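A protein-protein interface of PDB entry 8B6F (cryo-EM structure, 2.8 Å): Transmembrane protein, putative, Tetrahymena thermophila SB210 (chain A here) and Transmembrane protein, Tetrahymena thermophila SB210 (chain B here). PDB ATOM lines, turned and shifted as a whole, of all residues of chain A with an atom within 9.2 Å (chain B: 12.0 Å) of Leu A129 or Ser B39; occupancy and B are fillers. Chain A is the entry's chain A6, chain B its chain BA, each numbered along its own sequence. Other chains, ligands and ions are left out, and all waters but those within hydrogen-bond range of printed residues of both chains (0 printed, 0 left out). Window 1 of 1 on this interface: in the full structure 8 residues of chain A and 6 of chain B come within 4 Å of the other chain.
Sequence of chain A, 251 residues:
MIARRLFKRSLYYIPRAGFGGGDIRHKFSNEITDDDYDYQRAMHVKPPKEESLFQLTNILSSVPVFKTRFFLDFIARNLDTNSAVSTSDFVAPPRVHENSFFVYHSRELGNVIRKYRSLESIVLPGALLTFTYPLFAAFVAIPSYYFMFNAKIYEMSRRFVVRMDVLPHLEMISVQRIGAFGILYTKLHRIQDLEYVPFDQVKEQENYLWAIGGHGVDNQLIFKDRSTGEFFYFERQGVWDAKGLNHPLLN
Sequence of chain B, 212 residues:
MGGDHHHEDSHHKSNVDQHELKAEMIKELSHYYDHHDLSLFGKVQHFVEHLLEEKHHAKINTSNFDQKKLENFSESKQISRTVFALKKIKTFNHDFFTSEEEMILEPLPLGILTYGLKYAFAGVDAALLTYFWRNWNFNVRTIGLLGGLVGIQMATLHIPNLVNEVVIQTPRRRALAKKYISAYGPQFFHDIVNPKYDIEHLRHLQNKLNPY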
ATOM      1  N   SER A 121     -15.372  -3.362  14.731  1.00  0.00           N
ATOM      2  CA  SER A 121     -15.047  -3.760  16.093  1.00  0.00           C
ATOM      3  C   SER A 121     -14.968  -5.269  16.274  1.00  0.00           C
ATOM      4  O   SER A 121     -14.549  -5.724  17.342  1.00  0.00           O
ATOM      5  CB  SER A 121     -16.088  -3.198  17.069  1.00  0.00           C
ATOM      6  OG  SER A 121     -16.163  -1.787  16.982  1.00  0.00           O
ATOM      7  N   ILE A 122     -15.363  -6.051  15.269  1.00  0.00           N
ATOM      8  CA  ILE A 122     -15.372  -7.507  15.347  1.00  0.00           C
ATOM      9  C   ILE A 122     -14.555  -8.127  14.219  1.00  0.00           C
ATOM     10  O   ILE A 122     -13.660  -8.942  14.459  1.00  0.00           O
ATOM     11  CB  ILE A 122     -16.819  -8.063  15.353  1.00  0.00           C
ATOM     12  CG1 ILE A 122     -16.828  -9.596  15.311  1.00  0.00           C
ATOM     13  CG2 ILE A 122     -17.641  -7.515  14.190  1.00  0.00           C
ATOM     14  CD1 ILE A 122     -16.018 -10.251  16.398  1.00  0.00           C
ATOM     15  N   VAL A 123     -14.851  -7.749  12.976  1.00  0.00           N
ATOM     16  CA  VAL A 123     -14.136  -8.309  11.836  1.00  0.00           C
ATOM     17  C   VAL A 123     -12.667  -7.909  11.871  1.00  0.00           C
ATOM     18  O   VAL A 123     -11.780  -8.727  11.604  1.00  0.00           O
ATOM     19  CB  VAL A 123     -14.817  -7.872  10.525  1.00  0.00           C
ATOM     20  CG1 VAL A 123     -13.881  -8.044   9.347  1.00  0.00           C
ATOM     21  CG2 VAL A 123     -16.100  -8.660  10.307  1.00  0.00           C
ATOM     22  N   LEU A 124     -12.384  -6.640  12.193  1.00  0.00           N
ATOM     23  CA  LEU A 124     -11.007  -6.155  12.087  1.00  0.00           C
ATOM     24  C   LEU A 124     -10.103  -6.801  13.130  1.00  0.00           C
ATOM     25  O   LEU A 124      -9.119  -7.458  12.749  1.00  0.00           O
ATOM     26  CB  LEU A 124     -10.989  -4.627  12.149  1.00  0.00           C
ATOM     27  CG  LEU A 124      -9.649  -3.955  12.452  1.00  0.00           C
ATOM     28  CD1 LEU A 124      -8.643  -4.251  11.352  1.00  0.00           C
ATOM     29  CD2 LEU A 124      -9.838  -2.461  12.625  1.00  0.00           C
ATOM     30  N   PRO A 125     -10.355  -6.664  14.436  1.00  0.00           N
ATOM     31  CA  PRO A 125      -9.529  -7.415  15.398  1.00  0.00           C
ATOM     32  C   PRO A 125      -9.589  -8.913  15.176  1.00  0.00           C
ATOM     33  O   PRO A 125      -8.570  -9.601  15.310  1.00  0.00           O
ATOM     34  CB  PRO A 125     -10.114  -7.017  16.760  1.00  0.00           C
ATOM     35  CG  PRO A 125     -10.823  -5.751  16.523  1.00  0.00           C
ATOM     36  CD  PRO A 125     -11.340  -5.808  15.121  1.00  0.00           C
ATOM     37  N   GLY A 126     -10.763  -9.439  14.833  1.00  0.00           N
ATOM     38  CA  GLY A 126     -10.868 -10.857  14.540  1.00  0.00           C
ATOM     39  C   GLY A 126     -10.033 -11.259  13.341  1.00  0.00           C
ATOM     40  O   GLY A 126      -9.391 -12.311  13.342  1.00  0.00           O
ATOM     41  N   ALA A 127     -10.037 -10.430  12.297  1.00  0.00           N
ATOM     42  CA  ALA A 127      -9.186 -10.697  11.144  1.00  0.00           C
ATOM     43  C   ALA A 127      -7.715 -10.692  11.537  1.00  0.00           C
ATOM     44  O   ALA A 127      -6.946 -11.557  11.100  1.00  0.00           O
ATOM     45  CB  ALA A 127      -9.450  -9.663  10.052  1.00  0.00           C
ATOM     46  N   LEU A 128      -7.301  -9.723  12.357  1.00  0.00           N
ATOM     47  CA  LEU A 128      -5.904  -9.664  12.775  1.00  0.00           C
ATOM     48  C   LEU A 128      -5.498 -10.915  13.541  1.00  0.00           C
ATOM     49  O   LEU A 128      -4.415 -11.466  13.314  1.00  0.00           O
ATOM     50  CB  LEU A 128      -5.661  -8.425  13.637  1.00  0.00           C
ATOM     51  CG  LEU A 128      -4.280  -8.372  14.304  1.00  0.00           C
ATOM     52  CD1 LEU A 128      -3.182  -8.372  13.256  1.00  0.00           C
ATOM     53  CD2 LEU A 128      -4.140  -7.164  15.201  1.00  0.00           C
ATOM     54  N   LEU A 129      -6.350 -11.379  14.450  1.00  0.00           N
ATOM     55  CA  LEU A 129      -6.014 -12.503  15.311  1.00  0.00           C
ATOM     56  C   LEU A 129      -6.294 -13.855  14.672  1.00  0.00           C
ATOM     57  O   LEU A 129      -5.893 -14.879  15.233  1.00  0.00           O
ATOM     58  CB  LEU A 129      -6.790 -12.405  16.629  1.00  0.00           C
ATOM     59  CG  LEU A 129      -6.602 -11.114  17.430  1.00  0.00           C
ATOM     60  CD1 LEU A 129      -7.399 -11.165  18.724  1.00  0.00           C
ATOM     61  CD2 LEU A 129      -5.133 -10.846  17.712  1.00  0.00           C
ATOM     62  N   THR A 130      -6.968 -13.890  13.526  1.00  0.00           N
ATOM     63  CA  THR A 130      -7.357 -15.143  12.894  1.00  0.00           C
ATOM     64  C   THR A 130      -6.690 -15.397  11.554  1.00  0.00           C
ATOM     65  O   THR A 130      -6.308 -16.533  11.272  1.00  0.00           O
ATOM     66  CB  THR A 130      -8.869 -15.168  12.678  1.00  0.00           C
ATOM     67  OG1 THR A 130      -9.533 -14.825  13.900  1.00  0.00           O
ATOM     68  CG2 THR A 130      -9.295 -16.537  12.224  1.00  0.00           C
ATOM     69  N   PHE A 131      -6.566 -14.381  10.709  1.00  0.00           N
ATOM     70  CA  PHE A 131      -6.007 -14.596   9.384  1.00  0.00           C
ATOM     71  C   PHE A 131      -4.524 -14.923   9.478  1.00  0.00           C
ATOM     72  O   PHE A 131      -3.792 -14.349  10.287  1.00  0.00           O
ATOM     73  CB  PHE A 131      -6.235 -13.365   8.503  1.00  0.00           C
ATOM     74  CG  PHE A 131      -7.684 -13.099   8.183  1.00  0.00           C
ATOM     75  CD1 PHE A 131      -8.672 -14.024   8.498  1.00  0.00           C
ATOM     76  CD2 PHE A 131      -8.056 -11.924   7.553  1.00  0.00           C
ATOM     77  CE1 PHE A 131      -9.997 -13.774   8.198  1.00  0.00           C
ATOM     78  CE2 PHE A 131      -9.380 -11.670   7.250  1.00  0.00           C
ATOM     79  CZ  PHE A 131     -10.351 -12.596   7.572  1.00  0.00           C
ATOM     80  N   THR A 132      -4.085 -15.866   8.643  1.00  0.00           N
ATOM     81  CA  THR A 132      -2.674 -16.227   8.608  1.00  0.00           C
ATOM     82  C   THR A 132      -1.820 -15.093   8.062  1.00  0.00           C
ATOM     83  O   THR A 132      -0.652 -14.962   8.443  1.00  0.00           O
ATOM     84  CB  THR A 132      -2.478 -17.484   7.758  1.00  0.00           C
ATOM     85  OG1 THR A 132      -3.294 -18.545   8.268  1.00  0.00           O
ATOM     86  CG2 THR A 132      -1.021 -17.920   7.761  1.00  0.00           C
ATOM     87  N   TYR A 133      -2.377 -14.272   7.173  1.00  0.00           N
ATOM     88  CA  TYR A 133      -1.646 -13.193   6.511  1.00  0.00           C
ATOM     89  C   TYR A 133      -2.441 -11.903   6.642  1.00  0.00           C
ATOM     90  O   TYR A 133      -3.094 -11.459   5.688  1.00  0.00           O
ATOM     91  CB  TYR A 133      -1.372 -13.541   5.049  1.00  0.00           C
ATOM     92  CG  TYR A 133      -0.648 -14.855   4.892  1.00  0.00           C
ATOM     93  CD1 TYR A 133       0.631 -15.029   5.401  1.00  0.00           C
ATOM     94  CD2 TYR A 133      -1.244 -15.923   4.239  1.00  0.00           C
ATOM     95  CE1 TYR A 133       1.296 -16.228   5.264  1.00  0.00           C
ATOM     96  CE2 TYR A 133      -0.586 -17.128   4.095  1.00  0.00           C
ATOM     97  CZ  TYR A 133       0.684 -17.274   4.610  1.00  0.00           C
ATOM     98  OH  TYR A 133       1.342 -18.472   4.469  1.00  0.00           O
ATOM     99  N   PRO A 134      -2.413 -11.273   7.818  1.00  0.00           N
ATOM    100  CA  PRO A 134      -3.101  -9.980   7.968  1.00  0.00           C
ATOM    101  C   PRO A 134      -2.605  -8.921   7.002  1.00  0.00           C
ATOM    102  O   PRO A 134      -3.397  -8.079   6.563  1.00  0.00           O
ATOM    103  CB  PRO A 134      -2.813  -9.597   9.427  1.00  0.00           C
ATOM    104  CG  PRO A 134      -2.484 -10.877  10.105  1.00  0.00           C
ATOM    105  CD  PRO A 134      -1.801 -11.722   9.079  1.00  0.00           C
ATOM    106  N   HIS B  35       6.249 -27.602  10.076  1.00  0.00           N
ATOM    107  CA  HIS B  35       5.883 -26.231  10.404  1.00  0.00           C
ATOM    108  C   HIS B  35       4.955 -25.684   9.331  1.00  0.00           C
ATOM    109  O   HIS B  35       5.244 -25.804   8.137  1.00  0.00           O
ATOM    110  CB  HIS B  35       7.121 -25.338  10.527  1.00  0.00           C
ATOM    111  CG  HIS B  35       6.798 -23.885  10.693  1.00  0.00           C
ATOM    112  ND1 HIS B  35       6.637 -23.032   9.623  1.00  0.00           N
ATOM    113  CD2 HIS B  35       6.599 -23.137  11.804  1.00  0.00           C
ATOM    114  CE1 HIS B  35       6.355 -21.820  10.066  1.00  0.00           C
ATOM    115  NE2 HIS B  35       6.326 -21.856  11.386  1.00  0.00           N
ATOM    116  N   HIS B  36       3.850 -25.085   9.760  1.00  0.00           N
ATOM    117  CA  HIS B  36       2.910 -24.411   8.878  1.00  0.00           C
ATOM    118  C   HIS B  36       2.786 -22.953   9.291  1.00  0.00           C
ATOM    119  O   HIS B  36       3.308 -22.526  10.324  1.00  0.00           O
ATOM    120  CB  HIS B  36       1.533 -25.087   8.907  1.00  0.00           C
ATOM    121  CG  HIS B  36       1.550 -26.512   8.450  1.00  0.00           C
ATOM    122  ND1 HIS B  36       1.558 -27.575   9.329  1.00  0.00           N
ATOM    123  CD2 HIS B  36       1.568 -27.051   7.208  1.00  0.00           C
ATOM    124  CE1 HIS B  36       1.575 -28.706   8.647  1.00  0.00           C
ATOM    125  NE2 HIS B  36       1.583 -28.416   7.358  1.00  0.00           N
ATOM    126  N   ASP B  37       2.092 -22.180   8.462  1.00  0.00           N
ATOM    127  CA  ASP B  37       1.827 -20.777   8.751  1.00  0.00           C
ATOM    128  C   ASP B  37       0.528 -20.676   9.540  1.00  0.00           C
ATOM    129  O   ASP B  37      -0.531 -21.083   9.054  1.00  0.00           O
ATOM    130  CB  ASP B  37       1.737 -19.966   7.460  1.00  0.00           C
ATOM    131  CG  ASP B  37       3.037 -19.957   6.685  1.00  0.00           C
ATOM    132  OD1 ASP B  37       4.109 -20.055   7.318  1.00  0.00           O
ATOM    133  OD2 ASP B  37       2.989 -19.851   5.443  1.00  0.00           O
ATOM    134  N   LEU B  38       0.612 -20.139  10.754  1.00  0.00           N
ATOM    135  CA  LEU B  38      -0.542 -19.980  11.622  1.00  0.00           C
ATOM    136  C   LEU B  38      -0.729 -18.511  11.968  1.00  0.00           C
ATOM    137  O   LEU B  38       0.222 -17.725  11.940  1.00  0.00           O
ATOM    138  CB  LEU B  38      -0.394 -20.791  12.917  1.00  0.00           C
ATOM    139  CG  LEU B  38      -0.322 -22.318  12.810  1.00  0.00           C
ATOM    140  CD1 LEU B  38       1.031 -22.783  12.297  1.00  0.00           C
ATOM    141  CD2 LEU B  38      -0.627 -22.963  14.148  1.00  0.00           C
ATOM    142  N   SER B  39      -1.965 -18.144  12.289  1.00  0.00           N
ATOM    143  CA  SER B  39      -2.259 -16.802  12.767  1.00  0.00           C
ATOM    144  C   SER B  39      -1.802 -16.690  14.219  1.00  0.00           C
ATOM    145  O   SER B  39      -1.181 -17.601  14.771  1.00  0.00           O
ATOM    146  CB  SER B  39      -3.743 -16.497  12.599  1.00  0.00           C
ATOM    147  OG  SER B  39      -4.543 -17.479  13.233  1.00  0.00           O
ATOM    148  N   LEU B  40      -2.111 -15.565  14.866  1.00  0.00           N
ATOM    149  CA  LEU B  40      -1.762 -15.421  16.274  1.00  0.00           C
ATOM    150  C   LEU B  40      -2.517 -16.435  17.123  1.00  0.00           C
ATOM    151  O   LEU B  40      -1.933 -17.081  17.999  1.00  0.00           O
ATOM    152  CB  LEU B  40      -2.045 -13.996  16.745  1.00  0.00           C
ATOM    153  CG  LEU B  40      -1.329 -12.889  15.964  1.00  0.00           C
ATOM    154  CD1 LEU B  40      -1.690 -11.525  16.521  1.00  0.00           C
ATOM    155  CD2 LEU B  40       0.181 -13.085  15.975  1.00  0.00           C
ATOM    156  N   PHE B  41      -3.817 -16.594  16.872  1.00  0.00           N
ATOM    157  CA  PHE B  41      -4.590 -17.589  17.606  1.00  0.00           C
ATOM    158  C   PHE B  41      -4.081 -18.995  17.319  1.00  0.00           C
ATOM    159  O   PHE B  41      -3.978 -19.825  18.229  1.00  0.00           O
ATOM    160  CB  PHE B  41      -6.072 -17.471  17.247  1.00  0.00           C
ATOM    161  CG  PHE B  41      -6.945 -18.458  17.961  1.00  0.00           C
ATOM    162  CD1 PHE B  41      -7.476 -18.162  19.203  1.00  0.00           C
ATOM    163  CD2 PHE B  41      -7.239 -19.683  17.385  1.00  0.00           C
ATOM    164  CE1 PHE B  41      -8.281 -19.072  19.862  1.00  0.00           C
ATOM    165  CE2 PHE B  41      -8.043 -20.595  18.036  1.00  0.00           C
ATOM    166  CZ  PHE B  41      -8.566 -20.291  19.275  1.00  0.00           C
ATOM    167  N   GLY B  42      -3.757 -19.281  16.059  1.00  0.00           N
ATOM    168  CA  GLY B  42      -3.213 -20.586  15.725  1.00  0.00           C
ATOM    169  C   GLY B  42      -1.891 -20.855  16.416  1.00  0.00           C
ATOM    170  O   GLY B  42      -1.640 -21.967  16.888  1.00  0.00           O
ATOM    171  N   LYS B  43      -1.026 -19.841  16.486  1.00  0.00           N
ATOM    172  CA  LYS B  43       0.249 -20.007  17.175  1.00  0.00           C
ATOM    173  C   LYS B  43       0.049 -20.247  18.667  1.00  0.00           C
ATOM    174  O   LYS B  43       0.750 -21.070  19.266  1.00  0.00           O
ATOM    175  CB  LYS B  43       1.130 -18.781  16.939  1.00  0.00           C
ATOM    176  CG  LYS B  43       1.677 -18.688  15.521  1.00  0.00           C
ATOM    177  CD  LYS B  43       2.446 -17.395  15.300  1.00  0.00           C
ATOM    178  CE  LYS B  43       3.007 -17.329  13.887  1.00  0.00           C
ATOM    179  NZ  LYS B  43       3.720 -16.049  13.629  1.00  0.00           N
ATOM    180  N   VAL B  44      -0.894 -19.535  19.287  1.00  0.00           N
ATOM    181  CA  VAL B  44      -1.171 -19.762  20.704  1.00  0.00           C
ATOM    182  C   VAL B  44      -1.687 -21.179  20.923  1.00  0.00           C
ATOM    183  O   VAL B  44      -1.275 -21.866  21.865  1.00  0.00           O
ATOM    184  CB  VAL B  44      -2.165 -18.709  21.229  1.00  0.00           C
ATOM    185  CG1 VAL B  44      -2.637 -19.058  22.638  1.00  0.00           C
ATOM    186  CG2 VAL B  44      -1.530 -17.330  21.209  1.00  0.00           C
ATOM    187  N   GLN B  45      -2.596 -21.637  20.062  1.00  0.00           N
ATOM    188  CA  GLN B  45      -3.119 -22.993  20.193  1.00  0.00           C
ATOM    189  C   GLN B  45      -2.015 -24.023  19.995  1.00  0.00           C
ATOM    190  O   GLN B  45      -1.956 -25.030  20.710  1.00  0.00           O
ATOM    191  CB  GLN B  45      -4.250 -23.216  19.191  1.00  0.00           C
ATOM    192  CG  GLN B  45      -4.997 -24.527  19.385  1.00  0.00           C
ATOM    193  CD  GLN B  45      -6.192 -24.654  18.462  1.00  0.00           C
ATOM    194  OE1 GLN B  45      -6.379 -23.847  17.553  1.00  0.00           O
ATOM    195  NE2 GLN B  45      -7.013 -25.672  18.695  1.00  0.00           N
ATOM    196  N   HIS B  46      -1.130 -23.785  19.027  1.00  0.00           N
ATOM    197  CA  HIS B  46      -0.007 -24.689  18.803  1.00  0.00           C
ATOM    198  C   HIS B  46       0.924 -24.708  20.009  1.00  0.00           C
ATOM    199  O   HIS B  46       1.440 -25.765  20.389  1.00  0.00           O
ATOM    200  CB  HIS B  46       0.748 -24.276  17.541  1.00  0.00           C
ATOM    201  CG  HIS B  46       1.874 -25.194  17.181  1.00  0.00           C
ATOM    202  ND1 HIS B  46       3.192 -24.892  17.446  1.00  0.00           N
ATOM    203  CD2 HIS B  46       1.878 -26.404  16.576  1.00  0.00           C
ATOM    204  CE1 HIS B  46       3.961 -25.878  17.019  1.00  0.00           C
ATOM    205  NE2 HIS B  46       3.189 -26.807  16.486  1.00  0.00           N
ATOM    206  N   PHE B  47       1.155 -23.544  20.620  1.00  0.00           N
ATOM    207  CA  PHE B  47       1.964 -23.493  21.833  1.00  0.00           C
ATOM    208  C   PHE B  47       1.326 -24.305  22.953  1.00  0.00           C
ATOM    209  O   PHE B  47       2.014 -25.047  23.662  1.00  0.00           O
ATOM    210  CB  PHE B  47       2.157 -22.038  22.261  1.00  0.00           C
ATOM    211  CG  PHE B  47       2.885 -21.877  23.566  1.00  0.00           C
ATOM    212  CD1 PHE B  47       4.268 -21.794  23.595  1.00  0.00           C
ATOM    213  CD2 PHE B  47       2.186 -21.787  24.759  1.00  0.00           C
ATOM    214  CE1 PHE B  47       4.942 -21.639  24.792  1.00  0.00           C
ATOM    215  CE2 PHE B  47       2.854 -21.631  25.960  1.00  0.00           C
ATOM    216  CZ  PHE B  47       4.235 -21.557  25.975  1.00  0.00           C
ATOM    217  N   VAL B  48       0.010 -24.179  23.126  1.00  0.00           N
ATOM    218  CA  VAL B  48      -0.681 -24.942  24.162  1.00  0.00           C
ATOM    219  C   VAL B  48      -0.566 -26.436  23.889  1.00  0.00           C
ATOM    220  O   VAL B  48      -0.321 -27.232  24.803  1.00  0.00           O
ATOM    221  CB  VAL B  48      -2.152 -24.495  24.264  1.00  0.00           C
ATOM    222  CG1 VAL B  48      -2.946 -25.426  25.178  1.00  0.00           C
ATOM    223  CG2 VAL B  48      -2.236 -23.063  24.764  1.00  0.00           C
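Of chain A, only Leu A129 (3.5 Å), Thr A130 (2.8 Å) and Phe A131 (3.2 Å) come within 4 Å of Ser B39.
No residue of chain B comes within 4 Å of Pro A125.
No residue of chain B comes within 4 Å of Gly A126.
No residue of chain B comes within 4 Å of Ala A127.
Thr A130 touches just one residue of chain B: Ser B39.
Of chain B, only Asp B37 (3.4 Å) comes within 4 Å of Thr A132.
No residue of chain A comes within 4 Å of Gly B42.
Of the printed residues of chain A, Phe B41 touches Leu A129.
Of the printed residues of chain B, Tyr A133 touches Asp B37.
The nearest residue of chain B that does not touch Leu A129 is Gly B42 (5.0 Å).
OG of Ser B39 lies within hydrogen-bond range of O of Thr A130, 2.8 Å away.
The backbone NH of Phe B41 is in hydrogen-bond range of the backbone carbonyl oxygen of Leu A129, 3.2 Å away.
OD2 of Asp B37 sits close to OH of Tyr A133 (2.4 Å).
Of the 14 printed residues of chain A, 5 touch a printed residue of chain B.
Hydrophobic or aromatic side chains of chain B that line the printed part of chain A: Leu B40 and Phe B41.
Among the printed residues, 7 pairs touch across the chains.
Among the printed residues, pairs that only touch across the chains: Leu A129 with Ser B39, Leu A129 with Leu B40, Phe A131 with Ser B39 and Thr A132 with Asp B37.
OG of Ser B39 lies within hydrogen-bond range of N of Gly B42 (3.4 Å).
OG1 of Thr A130 sits at hydrogen-bond distance from O of Gly A126 (2.6 Å).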
